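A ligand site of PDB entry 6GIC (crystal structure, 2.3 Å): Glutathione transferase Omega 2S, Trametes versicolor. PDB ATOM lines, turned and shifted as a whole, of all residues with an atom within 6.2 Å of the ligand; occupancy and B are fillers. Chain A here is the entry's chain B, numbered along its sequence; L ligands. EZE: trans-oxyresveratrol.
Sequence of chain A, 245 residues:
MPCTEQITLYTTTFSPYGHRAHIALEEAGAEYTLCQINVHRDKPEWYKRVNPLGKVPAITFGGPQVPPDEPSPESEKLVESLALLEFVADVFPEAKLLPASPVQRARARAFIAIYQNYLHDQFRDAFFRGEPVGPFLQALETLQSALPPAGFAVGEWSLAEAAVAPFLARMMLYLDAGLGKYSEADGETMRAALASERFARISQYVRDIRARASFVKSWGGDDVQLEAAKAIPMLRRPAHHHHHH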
ATOM      1  N   THR A  13       3.916 -25.469   9.726  1.00  0.00           N
ATOM      2  CA  THR A  13       2.854 -24.721  10.393  1.00  0.00           C
ATOM      3  C   THR A  13       2.013 -23.983   9.373  1.00  0.00           C
ATOM      4  O   THR A  13       2.523 -23.486   8.359  1.00  0.00           O
ATOM      5  CB  THR A  13       3.431 -23.742  11.407  1.00  0.00           C
ATOM      6  OG1 THR A  13       4.669 -24.266  11.900  1.00  0.00           O
ATOM      7  CG2 THR A  13       2.434 -23.550  12.600  1.00  0.00           C
ATOM      8  N   PHE A  14       0.706 -23.936   9.621  1.00  0.00           N
ATOM      9  CA  PHE A  14      -0.235 -23.249   8.758  1.00  0.00           C
ATOM     10  C   PHE A  14      -0.413 -23.904   7.390  1.00  0.00           C
ATOM     11  O   PHE A  14      -1.171 -23.367   6.571  1.00  0.00           O
ATOM     12  CB  PHE A  14       0.172 -21.786   8.529  1.00  0.00           C
ATOM     13  CG  PHE A  14       0.598 -21.077   9.793  1.00  0.00           C
ATOM     14  CD1 PHE A  14      -0.342 -20.778  10.764  1.00  0.00           C
ATOM     15  CD2 PHE A  14       1.919 -20.727  10.011  1.00  0.00           C
ATOM     16  CE1 PHE A  14       0.029 -20.136  11.951  1.00  0.00           C
ATOM     17  CE2 PHE A  14       2.295 -20.085  11.182  1.00  0.00           C
ATOM     18  CZ  PHE A  14       1.350 -19.793  12.158  1.00  0.00           C
ATOM     19  N   SER A  15       0.234 -25.045   7.123  1.00  0.00           N
ATOM     20  CA  SER A  15      -0.019 -25.786   5.885  1.00  0.00           C
ATOM     21  C   SER A  15      -1.502 -26.160   5.779  1.00  0.00           C
ATOM     22  O   SER A  15      -2.044 -26.785   6.707  1.00  0.00           O
ATOM     23  CB  SER A  15       0.818 -27.076   5.821  1.00  0.00           C
ATOM     24  OG  SER A  15       0.546 -27.836   4.638  1.00  0.00           O
ATOM     25  N   PRO A  16      -2.187 -25.816   4.691  1.00  0.00           N
ATOM     26  CA  PRO A  16      -3.551 -26.318   4.511  1.00  0.00           C
ATOM     27  C   PRO A  16      -3.606 -27.807   4.301  1.00  0.00           C
ATOM     28  O   PRO A  16      -4.620 -28.440   4.630  1.00  0.00           O
ATOM     29  CB  PRO A  16      -4.059 -25.560   3.275  1.00  0.00           C
ATOM     30  CG  PRO A  16      -2.830 -25.143   2.535  1.00  0.00           C
ATOM     31  CD  PRO A  16      -1.741 -24.983   3.557  1.00  0.00           C
ATOM     32  N   TYR A  17      -2.526 -28.390   3.763  1.00  0.00           N
ATOM     33  CA  TYR A  17      -2.474 -29.840   3.556  1.00  0.00           C
ATOM     34  C   TYR A  17      -2.453 -30.553   4.902  1.00  0.00           C
ATOM     35  O   TYR A  17      -3.205 -31.493   5.135  1.00  0.00           O
ATOM     36  CB  TYR A  17      -1.260 -30.243   2.693  1.00  0.00           C
ATOM     37  CG  TYR A  17      -1.295 -29.721   1.268  1.00  0.00           C
ATOM     38  CD1 TYR A  17      -2.041 -30.366   0.276  1.00  0.00           C
ATOM     39  CD2 TYR A  17      -0.590 -28.572   0.906  1.00  0.00           C
ATOM     40  CE1 TYR A  17      -2.074 -29.880  -1.032  1.00  0.00           C
ATOM     41  CE2 TYR A  17      -0.616 -28.091  -0.382  1.00  0.00           C
ATOM     42  CZ  TYR A  17      -1.361 -28.749  -1.348  1.00  0.00           C
ATOM     43  OH  TYR A  17      -1.388 -28.254  -2.636  1.00  0.00           O
ATOM     44  N   VAL A  39       7.683 -23.363   8.420  1.00  0.00           N
ATOM     45  CA  VAL A  39       7.791 -23.264   6.954  1.00  0.00           C
ATOM     46  C   VAL A  39       9.117 -22.633   6.567  1.00  0.00           C
ATOM     47  O   VAL A  39       9.835 -23.134   5.687  1.00  0.00           O
ATOM     48  CB  VAL A  39       6.617 -22.470   6.353  1.00  0.00           C
ATOM     49  CG1 VAL A  39       6.849 -22.218   4.851  1.00  0.00           C
ATOM     50  CG2 VAL A  39       5.261 -23.156   6.556  1.00  0.00           C
ATOM     51  N   TYR A 115     -13.288 -30.398  -6.172  1.00  0.00           N
ATOM     52  CA  TYR A 115     -12.372 -29.426  -5.601  1.00  0.00           C
ATOM     53  C   TYR A 115     -11.012 -29.520  -6.299  1.00  0.00           C
ATOM     54  O   TYR A 115     -10.490 -28.508  -6.770  1.00  0.00           O
ATOM     55  CB  TYR A 115     -12.214 -29.610  -4.073  1.00  0.00           C
ATOM     56  CG  TYR A 115     -11.105 -28.705  -3.640  1.00  0.00           C
ATOM     57  CD1 TYR A 115     -11.306 -27.343  -3.623  1.00  0.00           C
ATOM     58  CD2 TYR A 115      -9.839 -29.183  -3.387  1.00  0.00           C
ATOM     59  CE1 TYR A 115     -10.309 -26.486  -3.339  1.00  0.00           C
ATOM     60  CE2 TYR A 115      -8.796 -28.305  -3.065  1.00  0.00           C
ATOM     61  CZ  TYR A 115      -9.061 -26.950  -3.062  1.00  0.00           C
ATOM     62  OH  TYR A 115      -8.094 -26.011  -2.790  1.00  0.00           O
ATOM     63  N   LEU A 119     -11.155 -26.235  -8.623  1.00  0.00           N
ATOM     64  CA  LEU A 119     -10.909 -25.030  -7.841  1.00  0.00           C
ATOM     65  C   LEU A 119      -9.460 -24.957  -7.344  1.00  0.00           C
ATOM     66  O   LEU A 119      -8.874 -23.876  -7.319  1.00  0.00           O
ATOM     67  CB  LEU A 119     -11.878 -24.971  -6.679  1.00  0.00           C
ATOM     68  CG  LEU A 119     -11.799 -23.813  -5.677  1.00  0.00           C
ATOM     69  CD1 LEU A 119     -11.960 -22.456  -6.333  1.00  0.00           C
ATOM     70  CD2 LEU A 119     -12.869 -24.019  -4.631  1.00  0.00           C
ATOM     71  N   HIS A 120      -8.899 -26.091  -6.943  1.00  0.00           N
ATOM     72  CA  HIS A 120      -7.567 -26.095  -6.348  1.00  0.00           C
ATOM     73  C   HIS A 120      -6.574 -25.301  -7.197  1.00  0.00           C
ATOM     74  O   HIS A 120      -5.859 -24.437  -6.688  1.00  0.00           O
ATOM     75  CB  HIS A 120      -7.095 -27.549  -6.178  1.00  0.00           C
ATOM     76  CG  HIS A 120      -5.910 -27.728  -5.287  1.00  0.00           C
ATOM     77  ND1 HIS A 120      -5.885 -27.318  -3.974  1.00  0.00           N
ATOM     78  CD2 HIS A 120      -4.699 -28.302  -5.522  1.00  0.00           C
ATOM     79  CE1 HIS A 120      -4.706 -27.625  -3.438  1.00  0.00           C
ATOM     80  NE2 HIS A 120      -3.981 -28.226  -4.361  1.00  0.00           N
ATOM     81  N   ASP A 121      -6.550 -25.550  -8.505  1.00  0.00           N
ATOM     82  CA  ASP A 121      -5.579 -24.901  -9.369  1.00  0.00           C
ATOM     83  C   ASP A 121      -5.951 -23.462  -9.712  1.00  0.00           C
ATOM     84  O   ASP A 121      -5.048 -22.700 -10.087  1.00  0.00           O
ATOM     85  CB  ASP A 121      -5.370 -25.700 -10.658  1.00  0.00           C
ATOM     86  CG  ASP A 121      -4.532 -26.960 -10.437  1.00  0.00           C
ATOM     87  OD1 ASP A 121      -3.818 -27.013  -9.420  1.00  0.00           O
ATOM     88  OD2 ASP A 121      -4.602 -27.895 -11.272  1.00  0.00           O
ATOM     89  N   GLN A 122      -7.225 -23.071  -9.595  1.00  0.00           N
ATOM     90  CA  GLN A 122      -7.559 -21.677  -9.798  1.00  0.00           C
ATOM     91  C   GLN A 122      -7.259 -20.820  -8.585  1.00  0.00           C
ATOM     92  O   GLN A 122      -6.932 -19.644  -8.729  1.00  0.00           O
ATOM     93  CB  GLN A 122      -9.033 -21.512 -10.206  1.00  0.00           C
ATOM     94  CG  GLN A 122      -9.362 -21.991 -11.608  1.00  0.00           C
ATOM     95  CD  GLN A 122      -8.267 -21.682 -12.637  1.00  0.00           C
ATOM     96  OE1 GLN A 122      -7.877 -20.525 -12.851  1.00  0.00           O
ATOM     97  NE2 GLN A 122      -7.743 -22.748 -13.261  1.00  0.00           N
ATOM     98  N   PHE A 123      -7.355 -21.395  -7.382  1.00  0.00           N
ATOM     99  CA  PHE A 123      -6.831 -20.717  -6.190  1.00  0.00           C
ATOM    100  C   PHE A 123      -5.353 -20.338  -6.382  1.00  0.00           C
ATOM    101  O   PHE A 123      -4.949 -19.211  -6.113  1.00  0.00           O
ATOM    102  CB  PHE A 123      -7.042 -21.607  -4.961  1.00  0.00           C
ATOM    103  CG  PHE A 123      -6.537 -21.037  -3.639  1.00  0.00           C
ATOM    104  CD1 PHE A 123      -6.316 -19.677  -3.475  1.00  0.00           C
ATOM    105  CD2 PHE A 123      -6.322 -21.881  -2.548  1.00  0.00           C
ATOM    106  CE1 PHE A 123      -5.880 -19.163  -2.271  1.00  0.00           C
ATOM    107  CE2 PHE A 123      -5.878 -21.386  -1.322  1.00  0.00           C
ATOM    108  CZ  PHE A 123      -5.659 -20.021  -1.196  1.00  0.00           C
ATOM    109  N   ARG A 124      -4.545 -21.284  -6.858  1.00  0.00           N
ATOM    110  CA  ARG A 124      -3.127 -21.013  -7.092  1.00  0.00           C
ATOM    111  C   ARG A 124      -2.935 -20.013  -8.232  1.00  0.00           C
ATOM    112  O   ARG A 124      -2.129 -19.090  -8.114  1.00  0.00           O
ATOM    113  CB  ARG A 124      -2.391 -22.305  -7.394  1.00  0.00           C
ATOM    114  CG  ARG A 124      -0.999 -22.164  -8.008  1.00  0.00           C
ATOM    115  CD  ARG A 124      -0.967 -22.675  -9.440  1.00  0.00           C
ATOM    116  NE  ARG A 124      -0.371 -23.995  -9.507  1.00  0.00           N
ATOM    117  CZ  ARG A 124      -0.550 -24.871 -10.494  1.00  0.00           C
ATOM    118  NH1 ARG A 124      -1.350 -24.585 -11.538  1.00  0.00           N
ATOM    119  NH2 ARG A 124       0.071 -26.039 -10.423  1.00  0.00           N
ATOM    120  N   PHE A 128      -1.839 -16.759  -6.225  1.00  0.00           N
ATOM    121  CA  PHE A 128      -0.383 -16.869  -6.201  1.00  0.00           C
ATOM    122  C   PHE A 128       0.278 -16.553  -7.532  1.00  0.00           C
ATOM    123  O   PHE A 128       1.485 -16.319  -7.552  1.00  0.00           O
ATOM    124  CB  PHE A 128       0.041 -18.278  -5.775  1.00  0.00           C
ATOM    125  CG  PHE A 128      -0.357 -18.635  -4.359  1.00  0.00           C
ATOM    126  CD1 PHE A 128      -1.674 -18.963  -4.043  1.00  0.00           C
ATOM    127  CD2 PHE A 128       0.573 -18.647  -3.347  1.00  0.00           C
ATOM    128  CE1 PHE A 128      -2.032 -19.294  -2.737  1.00  0.00           C
ATOM    129  CE2 PHE A 128       0.213 -18.979  -2.065  1.00  0.00           C
ATOM    130  CZ  PHE A 128      -1.074 -19.305  -1.758  1.00  0.00           C
ATOM    131  N   PRO A 166      -9.628 -26.407   4.708  1.00  0.00           N
ATOM    132  CA  PRO A 166      -8.415 -25.609   4.826  1.00  0.00           C
ATOM    133  C   PRO A 166      -8.237 -24.654   3.664  1.00  0.00           C
ATOM    134  O   PRO A 166      -7.773 -23.526   3.851  1.00  0.00           O
ATOM    135  CB  PRO A 166      -7.306 -26.668   4.880  1.00  0.00           C
ATOM    136  CG  PRO A 166      -8.010 -27.896   5.353  1.00  0.00           C
ATOM    137  CD  PRO A 166      -9.322 -27.838   4.673  1.00  0.00           C
ATOM    138  N   PHE A 167      -8.607 -25.070   2.448  1.00  0.00           N
ATOM    139  CA  PHE A 167      -8.342 -24.242   1.287  1.00  0.00           C
ATOM    140  C   PHE A 167      -9.412 -23.166   1.088  1.00  0.00           C
ATOM    141  O   PHE A 167      -9.093 -21.987   0.899  1.00  0.00           O
ATOM    142  CB  PHE A 167      -8.168 -25.140   0.062  1.00  0.00           C
ATOM    143  CG  PHE A 167      -6.901 -25.949   0.117  1.00  0.00           C
ATOM    144  CD1 PHE A 167      -6.887 -27.178   0.753  1.00  0.00           C
ATOM    145  CD2 PHE A 167      -5.718 -25.460  -0.409  1.00  0.00           C
ATOM    146  CE1 PHE A 167      -5.721 -27.896   0.822  1.00  0.00           C
ATOM    147  CE2 PHE A 167      -4.539 -26.192  -0.348  1.00  0.00           C
ATOM    148  CZ  PHE A 167      -4.538 -27.409   0.271  1.00  0.00           C
ATOM    149  N   ARG A 170      -8.873 -20.367   3.674  1.00  0.00           N
ATOM    150  CA  ARG A 170      -7.765 -19.450   3.440  1.00  0.00           C
ATOM    151  C   ARG A 170      -8.072 -18.520   2.282  1.00  0.00           C
ATOM    152  O   ARG A 170      -7.769 -17.327   2.354  1.00  0.00           O
ATOM    153  CB  ARG A 170      -6.457 -20.209   3.167  1.00  0.00           C
ATOM    154  CG  ARG A 170      -5.787 -20.701   4.436  1.00  0.00           C
ATOM    155  CD  ARG A 170      -4.989 -21.947   4.207  1.00  0.00           C
ATOM    156  NE  ARG A 170      -4.209 -22.333   5.393  1.00  0.00           N
ATOM    157  CZ  ARG A 170      -4.641 -23.131   6.361  1.00  0.00           C
ATOM    158  NH1 ARG A 170      -5.855 -23.642   6.284  1.00  0.00           N
ATOM    159  NH2 ARG A 170      -3.858 -23.426   7.395  1.00  0.00           N
ATOM    160  N   MET A 171      -8.666 -19.034   1.208  1.00  0.00           N
ATOM    161  CA  MET A 171      -8.891 -18.166   0.060  1.00  0.00           C
ATOM    162  C   MET A 171      -9.913 -17.092   0.403  1.00  0.00           C
ATOM    163  O   MET A 171      -9.773 -15.950  -0.036  1.00  0.00           O
ATOM    164  CB  MET A 171      -9.285 -19.012  -1.172  1.00  0.00           C
ATOM    165  CG  MET A 171     -10.671 -19.578  -1.176  1.00  0.00           C
ATOM    166  SD  MET A 171     -11.067 -20.725  -2.582  1.00  0.00           S
ATOM    167  CE  MET A 171      -9.900 -22.089  -2.369  1.00  0.00           C
ATOM    168  N   TYR A 174      -7.985 -14.653   2.593  1.00  0.00           N
ATOM    169  CA  TYR A 174      -7.073 -13.843   1.790  1.00  0.00           C
ATOM    170  C   TYR A 174      -7.831 -12.791   1.006  1.00  0.00           C
ATOM    171  O   TYR A 174      -7.326 -11.689   0.788  1.00  0.00           O
ATOM    172  CB  TYR A 174      -6.283 -14.725   0.816  1.00  0.00           C
ATOM    173  CG  TYR A 174      -5.399 -15.759   1.439  1.00  0.00           C
ATOM    174  CD1 TYR A 174      -5.288 -15.879   2.805  1.00  0.00           C
ATOM    175  CD2 TYR A 174      -4.690 -16.640   0.639  1.00  0.00           C
ATOM    176  CE1 TYR A 174      -4.476 -16.844   3.374  1.00  0.00           C
ATOM    177  CE2 TYR A 174      -3.879 -17.599   1.195  1.00  0.00           C
ATOM    178  CZ  TYR A 174      -3.769 -17.705   2.561  1.00  0.00           C
ATOM    179  OH  TYR A 174      -2.948 -18.663   3.108  1.00  0.00           O
ATOM    180  N   ILE A 232       4.018 -15.078   3.256  1.00  0.00           N
ATOM    181  CA  ILE A 232       4.164 -15.920   2.070  1.00  0.00           C
ATOM    182  C   ILE A 232       4.520 -15.005   0.905  1.00  0.00           C
ATOM    183  O   ILE A 232       3.642 -14.291   0.406  1.00  0.00           O
ATOM    184  CB  ILE A 232       2.887 -16.705   1.773  1.00  0.00           C
ATOM    185  CG1 ILE A 232       2.645 -17.749   2.856  1.00  0.00           C
ATOM    186  CG2 ILE A 232       2.997 -17.402   0.432  1.00  0.00           C
ATOM    187  CD1 ILE A 232       1.253 -18.420   2.744  1.00  0.00           C
ATOM    188  N   LEU A 235       2.390 -14.397  -2.312  1.00  0.00           N
ATOM    189  CA  LEU A 235       1.107 -13.693  -2.291  1.00  0.00           C
ATOM    190  C   LEU A 235       1.203 -12.196  -2.541  1.00  0.00           C
ATOM    191  O   LEU A 235       0.170 -11.529  -2.590  1.00  0.00           O
ATOM    192  CB  LEU A 235       0.406 -13.948  -0.950  1.00  0.00           C
ATOM    193  CG  LEU A 235      -0.465 -15.204  -0.826  1.00  0.00           C
ATOM    194  CD1 LEU A 235      -1.246 -15.121   0.469  1.00  0.00           C
ATOM    195  CD2 LEU A 235      -1.455 -15.428  -2.015  1.00  0.00           C
HETATM  196  C4  EZE L   1      -0.803 -25.455  -4.200  1.00  0.00           C
HETATM  197  C5  EZE L   1      -1.971 -24.758  -3.875  1.00  0.00           C
HETATM  198  C6  EZE L   1      -2.104 -24.030  -2.597  1.00  0.00           C
HETATM  199  C7  EZE L   1      -1.200 -24.034  -1.641  1.00  0.00           C
HETATM  200  C8  EZE L   1      -1.246 -23.314  -0.389  1.00  0.00           C
HETATM  201  C10 EZE L   1      -0.149 -22.549   1.632  1.00  0.00           C
HETATM  202  C13 EZE L   1      -2.279 -21.647   1.021  1.00  0.00           C
HETATM  203  C15 EZE L   1      -2.323 -22.474  -0.087  1.00  0.00           C
HETATM  204  O1  EZE L   1      -1.643 -26.785  -7.502  1.00  0.00           O
HETATM  205  C2  EZE L   1      -1.724 -26.143  -6.301  1.00  0.00           C
HETATM  206  C3  EZE L   1      -0.676 -26.149  -5.391  1.00  0.00           C
HETATM  207  C9  EZE L   1      -0.162 -23.346   0.497  1.00  0.00           C
HETATM  208  O11 EZE L   1       0.838 -22.645   2.574  1.00  0.00           O
HETATM  209  C12 EZE L   1      -1.196 -21.674   1.894  1.00  0.00           C
HETATM  210  O14 EZE L   1      -3.232 -20.688   1.214  1.00  0.00           O
HETATM  211  C16 EZE L   1      -3.026 -24.795  -4.799  1.00  0.00           C
HETATM  212  O17 EZE L   1      -4.237 -24.212  -4.527  1.00  0.00           O
HETATM  213  C18 EZE L   1      -2.902 -25.470  -6.003  1.00  0.00           C
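The side-chain hydroxyl of Tyr 174 lies within hydrogen-bond range of an oxygen (O14) of the ligand, 2.8 Å away.
The guanidinium group (NH2) of Arg 124 is in hydrogen-bond range of an oxygen (O1) of the ligand, at 3.5 Å.
An oxygen (O17) of the ligand is in hydrogen-bond range of the backbone carbonyl oxygen of His 120.
The side-chain carboxylate of Asp 121 is in hydrogen-bond range of an oxygen (O1) of the ligand (2.9 Å).
Pro 16 touches the ligand (CD to C10, 3.5 Å).
Tyr 17 touches the ligand.
Phe 123 touches the ligand.
Phe 128 touches the ligand.
Phe 167 touches the ligand (CE2 to C6, 3.96 Å).
Arg 170 touches the ligand.
Hydrophobic or aromatic side chains within 4 Å of the ligand: Pro 16, His 120, Phe 123, Phe 128, Phe 167 and Tyr 174.
Ten residues have an atom within 4 Å of the ligand: Pro 16, Tyr 17, His 120, Asp 121, Phe 123, Arg 124, Phe 128, Phe 167, Arg 170 and Tyr 174.
The side-chain hydroxyl (OH) of Tyr 115 sits at hydrogen-bond distance from a ring nitrogen (ND1) of His 120, 2.8 Å away.
A ring nitrogen (NE2) of His 120 is in hydrogen-bond range of the side-chain hydroxyl (OH) of Tyr 17, 3.1 Å away.
OG of Ser 15 lies close to N of Tyr 17, at 3.2 Å.
The backbone carbonyl oxygen (O) of Phe 14 is in hydrogen-bond range of the guanidinium group (NH2) of Arg 170, at 2.8 Å.
The backbone carbonyl oxygen of Pro 166 is in hydrogen-bond range of the guanidinium group of Arg 170 (3.1 Å).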
